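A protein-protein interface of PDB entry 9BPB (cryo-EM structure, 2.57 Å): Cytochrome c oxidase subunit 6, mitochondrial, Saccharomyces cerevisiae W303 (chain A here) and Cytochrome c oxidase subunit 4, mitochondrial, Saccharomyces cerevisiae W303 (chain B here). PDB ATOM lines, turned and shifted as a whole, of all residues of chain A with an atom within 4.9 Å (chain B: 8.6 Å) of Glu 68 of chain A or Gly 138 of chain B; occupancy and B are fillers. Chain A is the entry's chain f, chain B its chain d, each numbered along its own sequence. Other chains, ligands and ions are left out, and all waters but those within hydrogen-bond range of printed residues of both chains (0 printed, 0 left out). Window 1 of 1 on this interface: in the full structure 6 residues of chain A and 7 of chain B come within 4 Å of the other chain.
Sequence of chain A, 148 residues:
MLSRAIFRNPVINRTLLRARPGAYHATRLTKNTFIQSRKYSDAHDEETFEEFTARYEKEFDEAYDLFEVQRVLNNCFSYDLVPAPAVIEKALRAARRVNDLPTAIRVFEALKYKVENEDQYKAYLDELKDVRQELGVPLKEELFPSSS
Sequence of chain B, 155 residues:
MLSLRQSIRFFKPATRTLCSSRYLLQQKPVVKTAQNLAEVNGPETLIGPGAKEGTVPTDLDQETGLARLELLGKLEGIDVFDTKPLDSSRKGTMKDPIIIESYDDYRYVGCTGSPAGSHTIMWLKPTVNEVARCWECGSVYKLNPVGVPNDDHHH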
ATOM      1  N   ALA A  63     -22.162  -5.871   9.691  1.00  0.00           N
ATOM      2  CA  ALA A  63     -20.986  -5.216  10.256  1.00  0.00           C
ATOM      3  C   ALA A  63     -20.970  -3.800   9.701  1.00  0.00           C
ATOM      4  O   ALA A  63     -20.641  -3.595   8.530  1.00  0.00           O
ATOM      5  CB  ALA A  63     -19.705  -5.967   9.906  1.00  0.00           C
ATOM      6  N   TYR A  64     -21.322  -2.831  10.542  1.00  0.00           N
ATOM      7  CA  TYR A  64     -21.669  -1.491  10.092  1.00  0.00           C
ATOM      8  C   TYR A  64     -20.509  -0.503  10.116  1.00  0.00           C
ATOM      9  O   TYR A  64     -20.695   0.645   9.702  1.00  0.00           O
ATOM     10  CB  TYR A  64     -22.821  -0.942  10.940  1.00  0.00           C
ATOM     11  CG  TYR A  64     -22.603  -1.074  12.434  1.00  0.00           C
ATOM     12  CD1 TYR A  64     -22.907  -2.257  13.099  1.00  0.00           C
ATOM     13  CD2 TYR A  64     -22.096  -0.018  13.178  1.00  0.00           C
ATOM     14  CE1 TYR A  64     -22.708  -2.382  14.455  1.00  0.00           C
ATOM     15  CE2 TYR A  64     -21.897  -0.137  14.537  1.00  0.00           C
ATOM     16  CZ  TYR A  64     -22.202  -1.320  15.170  1.00  0.00           C
ATOM     17  OH  TYR A  64     -22.002  -1.442  16.525  1.00  0.00           O
ATOM     18  N   ASP A  65     -19.326  -0.906  10.575  1.00  0.00           N
ATOM     19  CA  ASP A  65     -18.191   0.002  10.598  1.00  0.00           C
ATOM     20  C   ASP A  65     -16.906  -0.790  10.411  1.00  0.00           C
ATOM     21  O   ASP A  65     -16.915  -2.016  10.281  1.00  0.00           O
ATOM     22  CB  ASP A  65     -18.147   0.828  11.893  1.00  0.00           C
ATOM     23  CG  ASP A  65     -18.111  -0.033  13.149  1.00  0.00           C
ATOM     24  OD1 ASP A  65     -17.322  -0.997  13.211  1.00  0.00           O
ATOM     25  OD2 ASP A  65     -18.867   0.273  14.094  1.00  0.00           O
ATOM     26  N   LEU A  66     -15.789  -0.064  10.406  1.00  0.00           N
ATOM     27  CA  LEU A  66     -14.489  -0.698  10.237  1.00  0.00           C
ATOM     28  C   LEU A  66     -13.976  -1.294  11.543  1.00  0.00           C
ATOM     29  O   LEU A  66     -13.072  -2.133  11.515  1.00  0.00           O
ATOM     30  CB  LEU A  66     -13.509   0.330   9.664  1.00  0.00           C
ATOM     31  CG  LEU A  66     -12.160  -0.066   9.059  1.00  0.00           C
ATOM     32  CD1 LEU A  66     -11.786   0.964   8.011  1.00  0.00           C
ATOM     33  CD2 LEU A  66     -11.077  -0.146  10.099  1.00  0.00           C
ATOM     34  N   PHE A  67     -14.546  -0.889  12.681  1.00  0.00           N
ATOM     35  CA  PHE A  67     -14.209  -1.525  13.950  1.00  0.00           C
ATOM     36  C   PHE A  67     -14.892  -2.879  14.085  1.00  0.00           C
ATOM     37  O   PHE A  67     -14.336  -3.805  14.689  1.00  0.00           O
ATOM     38  CB  PHE A  67     -14.593  -0.611  15.114  1.00  0.00           C
ATOM     39  CG  PHE A  67     -14.262  -1.171  16.475  1.00  0.00           C
ATOM     40  CD1 PHE A  67     -15.168  -1.974  17.153  1.00  0.00           C
ATOM     41  CD2 PHE A  67     -13.047  -0.894  17.078  1.00  0.00           C
ATOM     42  CE1 PHE A  67     -14.865  -2.489  18.396  1.00  0.00           C
ATOM     43  CE2 PHE A  67     -12.740  -1.408  18.324  1.00  0.00           C
ATOM     44  CZ  PHE A  67     -13.651  -2.204  18.983  1.00  0.00           C
ATOM     45  N   GLU A  68     -16.103  -3.014  13.536  1.00  0.00           N
ATOM     46  CA  GLU A  68     -16.833  -4.272  13.660  1.00  0.00           C
ATOM     47  C   GLU A  68     -16.295  -5.325  12.698  1.00  0.00           C
ATOM     48  O   GLU A  68     -16.243  -6.512  13.039  1.00  0.00           O
ATOM     49  CB  GLU A  68     -18.322  -4.037  13.426  1.00  0.00           C
ATOM     50  CG  GLU A  68     -19.036  -3.402  14.609  1.00  0.00           C
ATOM     51  CD  GLU A  68     -18.997  -4.270  15.852  1.00  0.00           C
ATOM     52  OE1 GLU A  68     -19.836  -5.188  15.960  1.00  0.00           O
ATOM     53  OE2 GLU A  68     -18.130  -4.037  16.719  1.00  0.00           O
ATOM     54  N   VAL A  69     -15.898  -4.913  11.492  1.00  0.00           N
ATOM     55  CA  VAL A  69     -15.352  -5.862  10.525  1.00  0.00           C
ATOM     56  C   VAL A  69     -14.048  -6.455  11.039  1.00  0.00           C
ATOM     57  O   VAL A  69     -13.818  -7.667  10.943  1.00  0.00           O
ATOM     58  CB  VAL A  69     -15.164  -5.185   9.155  1.00  0.00           C
ATOM     59  CG1 VAL A  69     -14.450  -6.121   8.195  1.00  0.00           C
ATOM     60  CG2 VAL A  69     -16.505  -4.763   8.589  1.00  0.00           C
ATOM     61  N   GLN A  70     -13.175  -5.615  11.595  1.00  0.00           N
ATOM     62  CA  GLN A  70     -11.932  -6.115  12.162  1.00  0.00           C
ATOM     63  C   GLN A  70     -12.155  -6.848  13.477  1.00  0.00           C
ATOM     64  O   GLN A  70     -11.249  -7.543  13.948  1.00  0.00           O
ATOM     65  CB  GLN A  70     -10.945  -4.963  12.356  1.00  0.00           C
ATOM     66  CG  GLN A  70     -10.190  -4.591  11.091  1.00  0.00           C
ATOM     67  CD  GLN A  70      -9.111  -3.559  11.334  1.00  0.00           C
ATOM     68  OE1 GLN A  70      -9.393  -2.376  11.483  1.00  0.00           O
ATOM     69  NE2 GLN A  70      -7.863  -4.003  11.371  1.00  0.00           N
ATOM     70  N   ARG A  71     -13.336  -6.705  14.084  1.00  0.00           N
ATOM     71  CA  ARG A  71     -13.645  -7.471  15.287  1.00  0.00           C
ATOM     72  C   ARG A  71     -14.163  -8.861  14.937  1.00  0.00           C
ATOM     73  O   ARG A  71     -13.828  -9.843  15.612  1.00  0.00           O
ATOM     74  CB  ARG A  71     -14.664  -6.720  16.140  1.00  0.00           C
ATOM     75  CG  ARG A  71     -15.162  -7.502  17.345  1.00  0.00           C
ATOM     76  CD  ARG A  71     -16.338  -6.808  18.012  1.00  0.00           C
ATOM     77  NE  ARG A  71     -17.605  -7.120  17.359  1.00  0.00           N
ATOM     78  CZ  ARG A  71     -18.228  -8.286  17.446  1.00  0.00           C
ATOM     79  NH1 ARG A  71     -17.738  -9.281  18.167  1.00  0.00           N
ATOM     80  NH2 ARG A  71     -19.374  -8.460  16.793  1.00  0.00           N
ATOM     81  N   VAL A  72     -14.984  -8.965  13.889  1.00  0.00           N
ATOM     82  CA  VAL A  72     -15.535 -10.258  13.499  1.00  0.00           C
ATOM     83  C   VAL A  72     -14.451 -11.146  12.898  1.00  0.00           C
ATOM     84  O   VAL A  72     -14.358 -12.336  13.224  1.00  0.00           O
ATOM     85  CB  VAL A  72     -16.716 -10.068  12.531  1.00  0.00           C
ATOM     86  CG1 VAL A  72     -17.218 -11.409  12.034  1.00  0.00           C
ATOM     87  CG2 VAL A  72     -17.838  -9.307  13.211  1.00  0.00           C
ATOM     88  N   LYS B  91     -27.428  -5.711  23.556  1.00  0.00           N
ATOM     89  CA  LYS B  91     -26.016  -5.643  23.205  1.00  0.00           C
ATOM     90  C   LYS B  91     -25.520  -4.202  23.214  1.00  0.00           C
ATOM     91  O   LYS B  91     -24.545  -3.884  23.899  1.00  0.00           O
ATOM     92  CB  LYS B  91     -25.768  -6.280  21.834  1.00  0.00           C
ATOM     93  CG  LYS B  91     -24.453  -5.850  21.198  1.00  0.00           C
ATOM     94  CD  LYS B  91     -24.095  -6.697  19.989  1.00  0.00           C
ATOM     95  CE  LYS B  91     -23.568  -8.057  20.410  1.00  0.00           C
ATOM     96  NZ  LYS B  91     -22.882  -8.757  19.289  1.00  0.00           N
ATOM     97  N   GLY B  92     -26.189  -3.322  22.476  1.00  0.00           N
ATOM     98  CA  GLY B  92     -25.797  -1.928  22.429  1.00  0.00           C
ATOM     99  C   GLY B  92     -24.882  -1.626  21.263  1.00  0.00           C
ATOM    100  O   GLY B  92     -23.740  -2.092  21.225  1.00  0.00           O
ATOM    101  N   THR B  93     -25.367  -0.844  20.310  1.00  0.00           N
ATOM    102  CA  THR B  93     -24.640  -0.525  19.092  1.00  0.00           C
ATOM    103  C   THR B  93     -24.184   0.929  19.133  1.00  0.00           C
ATOM    104  O   THR B  93     -24.393   1.643  20.116  1.00  0.00           O
ATOM    105  CB  THR B  93     -25.508  -0.793  17.858  1.00  0.00           C
ATOM    106  OG1 THR B  93     -26.759  -0.113  17.996  1.00  0.00           O
ATOM    107  CG2 THR B  93     -25.765  -2.281  17.706  1.00  0.00           C
ATOM    108  N   MET B  94     -23.552   1.368  18.043  1.00  0.00           N
ATOM    109  CA  MET B  94     -23.088   2.749  17.963  1.00  0.00           C
ATOM    110  C   MET B  94     -24.258   3.724  17.934  1.00  0.00           C
ATOM    111  O   MET B  94     -24.175   4.823  18.492  1.00  0.00           O
ATOM    112  CB  MET B  94     -22.200   2.937  16.734  1.00  0.00           C
ATOM    113  CG  MET B  94     -21.150   4.019  16.896  1.00  0.00           C
ATOM    114  SD  MET B  94     -19.849   3.575  18.057  1.00  0.00           S
ATOM    115  CE  MET B  94     -18.657   4.867  17.720  1.00  0.00           C
ATOM    116  N   LYS B  95     -25.357   3.339  17.288  1.00  0.00           N
ATOM    117  CA  LYS B  95     -26.520   4.206  17.181  1.00  0.00           C
ATOM    118  C   LYS B  95     -27.530   3.998  18.301  1.00  0.00           C
ATOM    119  O   LYS B  95     -28.561   4.678  18.317  1.00  0.00           O
ATOM    120  CB  LYS B  95     -27.211   4.003  15.828  1.00  0.00           C
ATOM    121  CG  LYS B  95     -28.005   2.716  15.722  1.00  0.00           C
ATOM    122  CD  LYS B  95     -28.610   2.561  14.335  1.00  0.00           C
ATOM    123  CE  LYS B  95     -27.561   2.765  13.255  1.00  0.00           C
ATOM    124  NZ  LYS B  95     -28.149   2.720  11.889  1.00  0.00           N
ATOM    125  N   ASP B  96     -27.269   3.082  19.232  1.00  0.00           N
ATOM    126  CA  ASP B  96     -28.143   2.855  20.384  1.00  0.00           C
ATOM    127  C   ASP B  96     -27.294   2.415  21.569  1.00  0.00           C
ATOM    128  O   ASP B  96     -27.359   1.264  22.012  1.00  0.00           O
ATOM    129  CB  ASP B  96     -29.219   1.820  20.053  1.00  0.00           C
ATOM    130  CG  ASP B  96     -30.474   1.998  20.884  1.00  0.00           C
ATOM    131  OD1 ASP B  96     -30.499   2.908  21.739  1.00  0.00           O
ATOM    132  OD2 ASP B  96     -31.437   1.232  20.677  1.00  0.00           O
ATOM    133  N   PRO B  97     -26.480   3.319  22.111  1.00  0.00           N
ATOM    134  CA  PRO B  97     -25.601   2.941  23.222  1.00  0.00           C
ATOM    135  C   PRO B  97     -26.373   2.718  24.509  1.00  0.00           C
ATOM    136  O   PRO B  97     -27.469   3.247  24.708  1.00  0.00           O
ATOM    137  CB  PRO B  97     -24.659   4.141  23.348  1.00  0.00           C
ATOM    138  CG  PRO B  97     -25.472   5.286  22.865  1.00  0.00           C
ATOM    139  CD  PRO B  97     -26.349   4.746  21.769  1.00  0.00           C
ATOM    140  N   CYS B 111     -18.070  -5.462  31.074  1.00  0.00           N
ATOM    141  CA  CYS B 111     -18.912  -6.151  30.105  1.00  0.00           C
ATOM    142  C   CYS B 111     -18.619  -7.641  30.115  1.00  0.00           C
ATOM    143  O   CYS B 111     -17.454  -8.049  30.157  1.00  0.00           O
ATOM    144  CB  CYS B 111     -18.687  -5.597  28.703  1.00  0.00           C
ATOM    145  SG  CYS B 111     -19.749  -6.335  27.465  1.00  0.00           S
ATOM    146  N   GLY B 113     -21.279  -9.725  28.220  1.00  0.00           N
ATOM    147  CA  GLY B 113     -22.054 -10.206  27.092  1.00  0.00           C
ATOM    148  C   GLY B 113     -23.536 -10.036  27.338  1.00  0.00           C
ATOM    149  O   GLY B 113     -23.981  -9.730  28.443  1.00  0.00           O
ATOM    150  N   HIS B 119     -18.767 -14.098  27.755  1.00  0.00           N
ATOM    151  CA  HIS B 119     -17.330 -14.044  27.525  1.00  0.00           C
ATOM    152  C   HIS B 119     -16.628 -13.564  28.791  1.00  0.00           C
ATOM    153  O   HIS B 119     -17.234 -13.442  29.858  1.00  0.00           O
ATOM    154  CB  HIS B 119     -16.984 -13.155  26.319  1.00  0.00           C
ATOM    155  CG  HIS B 119     -17.349 -11.710  26.486  1.00  0.00           C
ATOM    156  ND1 HIS B 119     -16.706 -10.871  27.371  1.00  0.00           N
ATOM    157  CD2 HIS B 119     -18.273 -10.947  25.853  1.00  0.00           C
ATOM    158  CE1 HIS B 119     -17.227  -9.660  27.286  1.00  0.00           C
ATOM    159  NE2 HIS B 119     -18.179  -9.679  26.372  1.00  0.00           N
ATOM    160  N   MET B 122     -14.330  -7.480  30.313  1.00  0.00           N
ATOM    161  CA  MET B 122     -13.432  -6.476  29.756  1.00  0.00           C
ATOM    162  C   MET B 122     -13.795  -5.135  30.378  1.00  0.00           C
ATOM    163  O   MET B 122     -14.888  -4.613  30.140  1.00  0.00           O
ATOM    164  CB  MET B 122     -13.537  -6.423  28.232  1.00  0.00           C
ATOM    165  CG  MET B 122     -12.570  -5.453  27.577  1.00  0.00           C
ATOM    166  SD  MET B 122     -12.598  -5.545  25.781  1.00  0.00           S
ATOM    167  CE  MET B 122     -11.617  -4.110  25.354  1.00  0.00           C
ATOM    168  N   LEU B 124     -14.020  -1.261  30.976  1.00  0.00           N
ATOM    169  CA  LEU B 124     -14.087  -0.098  30.110  1.00  0.00           C
ATOM    170  C   LEU B 124     -14.187   1.160  30.958  1.00  0.00           C
ATOM    171  O   LEU B 124     -14.533   1.111  32.141  1.00  0.00           O
ATOM    172  CB  LEU B 124     -15.278  -0.185  29.147  1.00  0.00           C
ATOM    173  CG  LEU B 124     -15.404  -1.468  28.323  1.00  0.00           C
ATOM    174  CD1 LEU B 124     -16.703  -1.473  27.541  1.00  0.00           C
ATOM    175  CD2 LEU B 124     -14.216  -1.641  27.394  1.00  0.00           C
ATOM    176  N   ALA B 132     -16.959   3.811  25.004  1.00  0.00           N
ATOM    177  CA  ALA B 132     -16.247   2.540  24.997  1.00  0.00           C
ATOM    178  C   ALA B 132     -16.884   1.586  23.994  1.00  0.00           C
ATOM    179  O   ALA B 132     -18.091   1.632  23.745  1.00  0.00           O
ATOM    180  CB  ALA B 132     -16.243   1.921  26.392  1.00  0.00           C
ATOM    181  N   ARG B 133     -16.061   0.705  23.417  1.00  0.00           N
ATOM    182  CA  ARG B 133     -16.515  -0.132  22.318  1.00  0.00           C
ATOM    183  C   ARG B 133     -16.488  -1.630  22.579  1.00  0.00           C
ATOM    184  O   ARG B 133     -17.140  -2.366  21.832  1.00  0.00           O
ATOM    185  CB  ARG B 133     -15.699   0.148  21.047  1.00  0.00           C
ATOM    186  CG  ARG B 133     -15.858   1.552  20.514  1.00  0.00           C
ATOM    187  CD  ARG B 133     -17.271   1.759  20.006  1.00  0.00           C
ATOM    188  NE  ARG B 133     -17.624   0.851  18.921  1.00  0.00           N
ATOM    189  CZ  ARG B 133     -17.374   1.077  17.639  1.00  0.00           C
ATOM    190  NH1 ARG B 133     -16.742   2.168  17.241  1.00  0.00           N
ATOM    191  NH2 ARG B 133     -17.776   0.192  16.734  1.00  0.00           N
ATOM    192  N   CYS B 134     -15.764  -2.111  23.592  1.00  0.00           N
ATOM    193  CA  CYS B 134     -15.769  -3.531  23.953  1.00  0.00           C
ATOM    194  C   CYS B 134     -15.330  -4.404  22.769  1.00  0.00           C
ATOM    195  O   CYS B 134     -16.114  -5.134  22.163  1.00  0.00           O
ATOM    196  CB  CYS B 134     -17.141  -3.960  24.487  1.00  0.00           C
ATOM    197  SG  CYS B 134     -17.169  -5.631  25.173  1.00  0.00           S
ATOM    198  N   TRP B 135     -14.043  -4.274  22.446  1.00  0.00           N
ATOM    199  CA  TRP B 135     -13.381  -4.958  21.337  1.00  0.00           C
ATOM    200  C   TRP B 135     -13.748  -6.435  21.208  1.00  0.00           C
ATOM    201  O   TRP B 135     -13.666  -6.999  20.114  1.00  0.00           O
ATOM    202  CB  TRP B 135     -11.864  -4.805  21.498  1.00  0.00           C
ATOM    203  CG  TRP B 135     -11.027  -5.668  20.601  1.00  0.00           C
ATOM    204  CD1 TRP B 135     -10.275  -6.743  20.972  1.00  0.00           C
ATOM    205  CD2 TRP B 135     -10.831  -5.511  19.191  1.00  0.00           C
ATOM    206  NE1 TRP B 135      -9.637  -7.275  19.880  1.00  0.00           N
ATOM    207  CE2 TRP B 135      -9.961  -6.535  18.773  1.00  0.00           C
ATOM    208  CE3 TRP B 135     -11.311  -4.608  18.239  1.00  0.00           C
ATOM    209  CZ2 TRP B 135      -9.563  -6.682  17.447  1.00  0.00           C
ATOM    210  CZ3 TRP B 135     -10.915  -4.755  16.925  1.00  0.00           C
ATOM    211  CH2 TRP B 135     -10.052  -5.783  16.540  1.00  0.00           C
ATOM    212  N   GLU B 136     -14.150  -7.075  22.307  1.00  0.00           N
ATOM    213  CA  GLU B 136     -14.526  -8.483  22.236  1.00  0.00           C
ATOM    214  C   GLU B 136     -15.962  -8.659  21.747  1.00  0.00           C
ATOM    215  O   GLU B 136     -16.219  -9.450  20.834  1.00  0.00           O
ATOM    216  CB  GLU B 136     -14.345  -9.149  23.599  1.00  0.00           C
ATOM    217  CG  GLU B 136     -13.998 -10.627  23.522  1.00  0.00           C
ATOM    218  CD  GLU B 136     -15.175 -11.494  23.114  1.00  0.00           C
ATOM    219  OE1 GLU B 136     -16.329 -11.094  23.374  1.00  0.00           O
ATOM    220  OE2 GLU B 136     -14.948 -12.573  22.526  1.00  0.00           O
ATOM    221  N   CYS B 137     -16.910  -7.937  22.346  1.00  0.00           N
ATOM    222  CA  CYS B 137     -18.326  -8.107  22.041  1.00  0.00           C
ATOM    223  C   CYS B 137     -18.908  -7.008  21.166  1.00  0.00           C
ATOM    224  O   CYS B 137     -19.734  -7.305  20.303  1.00  0.00           O
ATOM    225  CB  CYS B 137     -19.142  -8.187  23.337  1.00  0.00           C
ATOM    226  SG  CYS B 137     -20.828  -8.797  23.121  1.00  0.00           S
ATOM    227  N   GLY B 138     -18.509  -5.756  21.361  1.00  0.00           N
ATOM    228  CA  GLY B 138     -18.958  -4.674  20.514  1.00  0.00           C
ATOM    229  C   GLY B 138     -19.962  -3.717  21.117  1.00  0.00           C
ATOM    230  O   GLY B 138     -20.486  -2.867  20.392  1.00  0.00           O
ATOM    231  N   SER B 139     -20.249  -3.826  22.412  1.00  0.00           N
ATOM    232  CA  SER B 139     -21.202  -2.930  23.048  1.00  0.00           C
ATOM    233  C   SER B 139     -20.653  -1.509  23.123  1.00  0.00           C
ATOM    234  O   SER B 139     -19.440  -1.289  23.155  1.00  0.00           O
ATOM    235  CB  SER B 139     -21.546  -3.431  24.448  1.00  0.00           C
ATOM    236  OG  SER B 139     -22.007  -4.770  24.404  1.00  0.00           O
ATOM    237  N   VAL B 140     -21.562  -0.538  23.154  1.00  0.00           N
ATOM    238  CA  VAL B 140     -21.214   0.879  23.172  1.00  0.00           C
ATOM    239  C   VAL B 140     -21.913   1.529  24.359  1.00  0.00           C
ATOM    240  O   VAL B 140     -23.093   1.262  24.611  1.00  0.00           O
ATOM    241  CB  VAL B 140     -21.606   1.575  21.856  1.00  0.00           C
ATOM    242  CG1 VAL B 140     -21.306   3.063  21.926  1.00  0.00           C
ATOM    243  CG2 VAL B 140     -20.884   0.938  20.685  1.00  0.00           C
ATOM    244  N   TYR B 141     -21.182   2.373  25.088  1.00  0.00           N
ATOM    245  CA  TYR B 141     -21.701   3.057  26.266  1.00  0.00           C
ATOM    246  C   TYR B 141     -21.445   4.551  26.149  1.00  0.00           C
ATOM    247  O   TYR B 141     -20.323   4.969  25.854  1.00  0.00           O
ATOM    248  CB  TYR B 141     -21.054   2.525  27.543  1.00  0.00           C
ATOM    249  CG  TYR B 141     -21.287   1.058  27.752  1.00  0.00           C
ATOM    250  CD1 TYR B 141     -20.419   0.125  27.216  1.00  0.00           C
ATOM    251  CD2 TYR B 141     -22.383   0.603  28.466  1.00  0.00           C
ATOM    252  CE1 TYR B 141     -20.629  -1.215  27.391  1.00  0.00           C
ATOM    253  CE2 TYR B 141     -22.602  -0.743  28.650  1.00  0.00           C
ATOM    254  CZ  TYR B 141     -21.719  -1.649  28.112  1.00  0.00           C
ATOM    255  OH  TYR B 141     -21.926  -2.997  28.289  1.00  0.00           O
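Among the printed residues, pairs that only touch across the chains: Tyr 64 of chain A with Thr 93 of chain B (3.8 Å), Tyr 64 of chain A with Met 94 of chain B (3.6 Å), Phe 67 of chain A with Arg 133 of chain B (3.4 Å), Phe 67 of chain A with Trp 135 of chain B (3.4 Å), Glu 68 of chain A with Gly 138 of chain B (3.9 Å), Gln 70 of chain A with Trp 135 of chain B (3.4 Å), Arg 71 of chain A with Trp 135 of chain B (3.2 Å) and Arg 71 of chain A with Cys 137 of chain B (3.4 Å).
Along chain B the printed residues that touch a printed residue of chain A span positions 93 to 138. Of the 10 printed residues of chain A, 6 touch a printed residue of chain B. Hydrophobic or aromatic side chains of chain A that line the printed part of chain B: Tyr 64 and Phe 67. Along chain A the printed residues that touch a printed residue of chain B span positions 64 to 71. Among the printed residues, 10 pairs touch across the chains.
Of the printed residues of chain B, Tyr 64 of chain A touches Thr 93 (3.8 Å) and Met 94 (3.6 Å). Glu 68 of chain A touches just one residue of chain B: Gly 138 (3.9 Å). Pro 97 of chain B touches none of the printed residues of chain A. Met 122 of chain B touches none of the printed residues of chain A. Printed residues of chain A within 4 Å of Cys 137 of chain B: Arg 71 (3.4 Å). Gly 138 of chain B touches just one residue of chain A: Glu 68. The nearest residue of chain A that does not touch Gly 138 of chain B is Arg 71 of chain A (4.1 Å).
The backbone carbonyl oxygen of Glu 136 of chain B sits at hydrogen-bond distance from the guanidinium group of Arg 71 of chain A, at 3.1 Å. NH2 of Arg 133 of chain B lies within salt-bridge range of OD2 of Asp 65 of chain A (2.9 Å).
OD1 of Asp 65 of chain A is in hydrogen-bond range of N of Phe 67 of chain A. The side-chain sulfur (SD) of Met 94 of chain B sits close to the guanidinium group (NH1) of Arg 133 of chain B, at 3.5 Å. The side-chain hydroxyl (OG1) of Thr 93 of chain B sits at hydrogen-bond distance from the backbone NH (N) of Asp 96 of chain B (3.5 Å). The backbone NH of Cys 137 of chain B lies close to the side-chain sulfur of Cys 134 of chain B. The side-chain carboxylate (OE2) of Glu 68 of chain A is in salt-bridge range of the guanidinium group (NE) of Arg 71 of chain A (3.2 Å). N of Ser 139 of chain B is in hydrogen-bond range of O of Arg 133 of chain B (3.5 Å).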
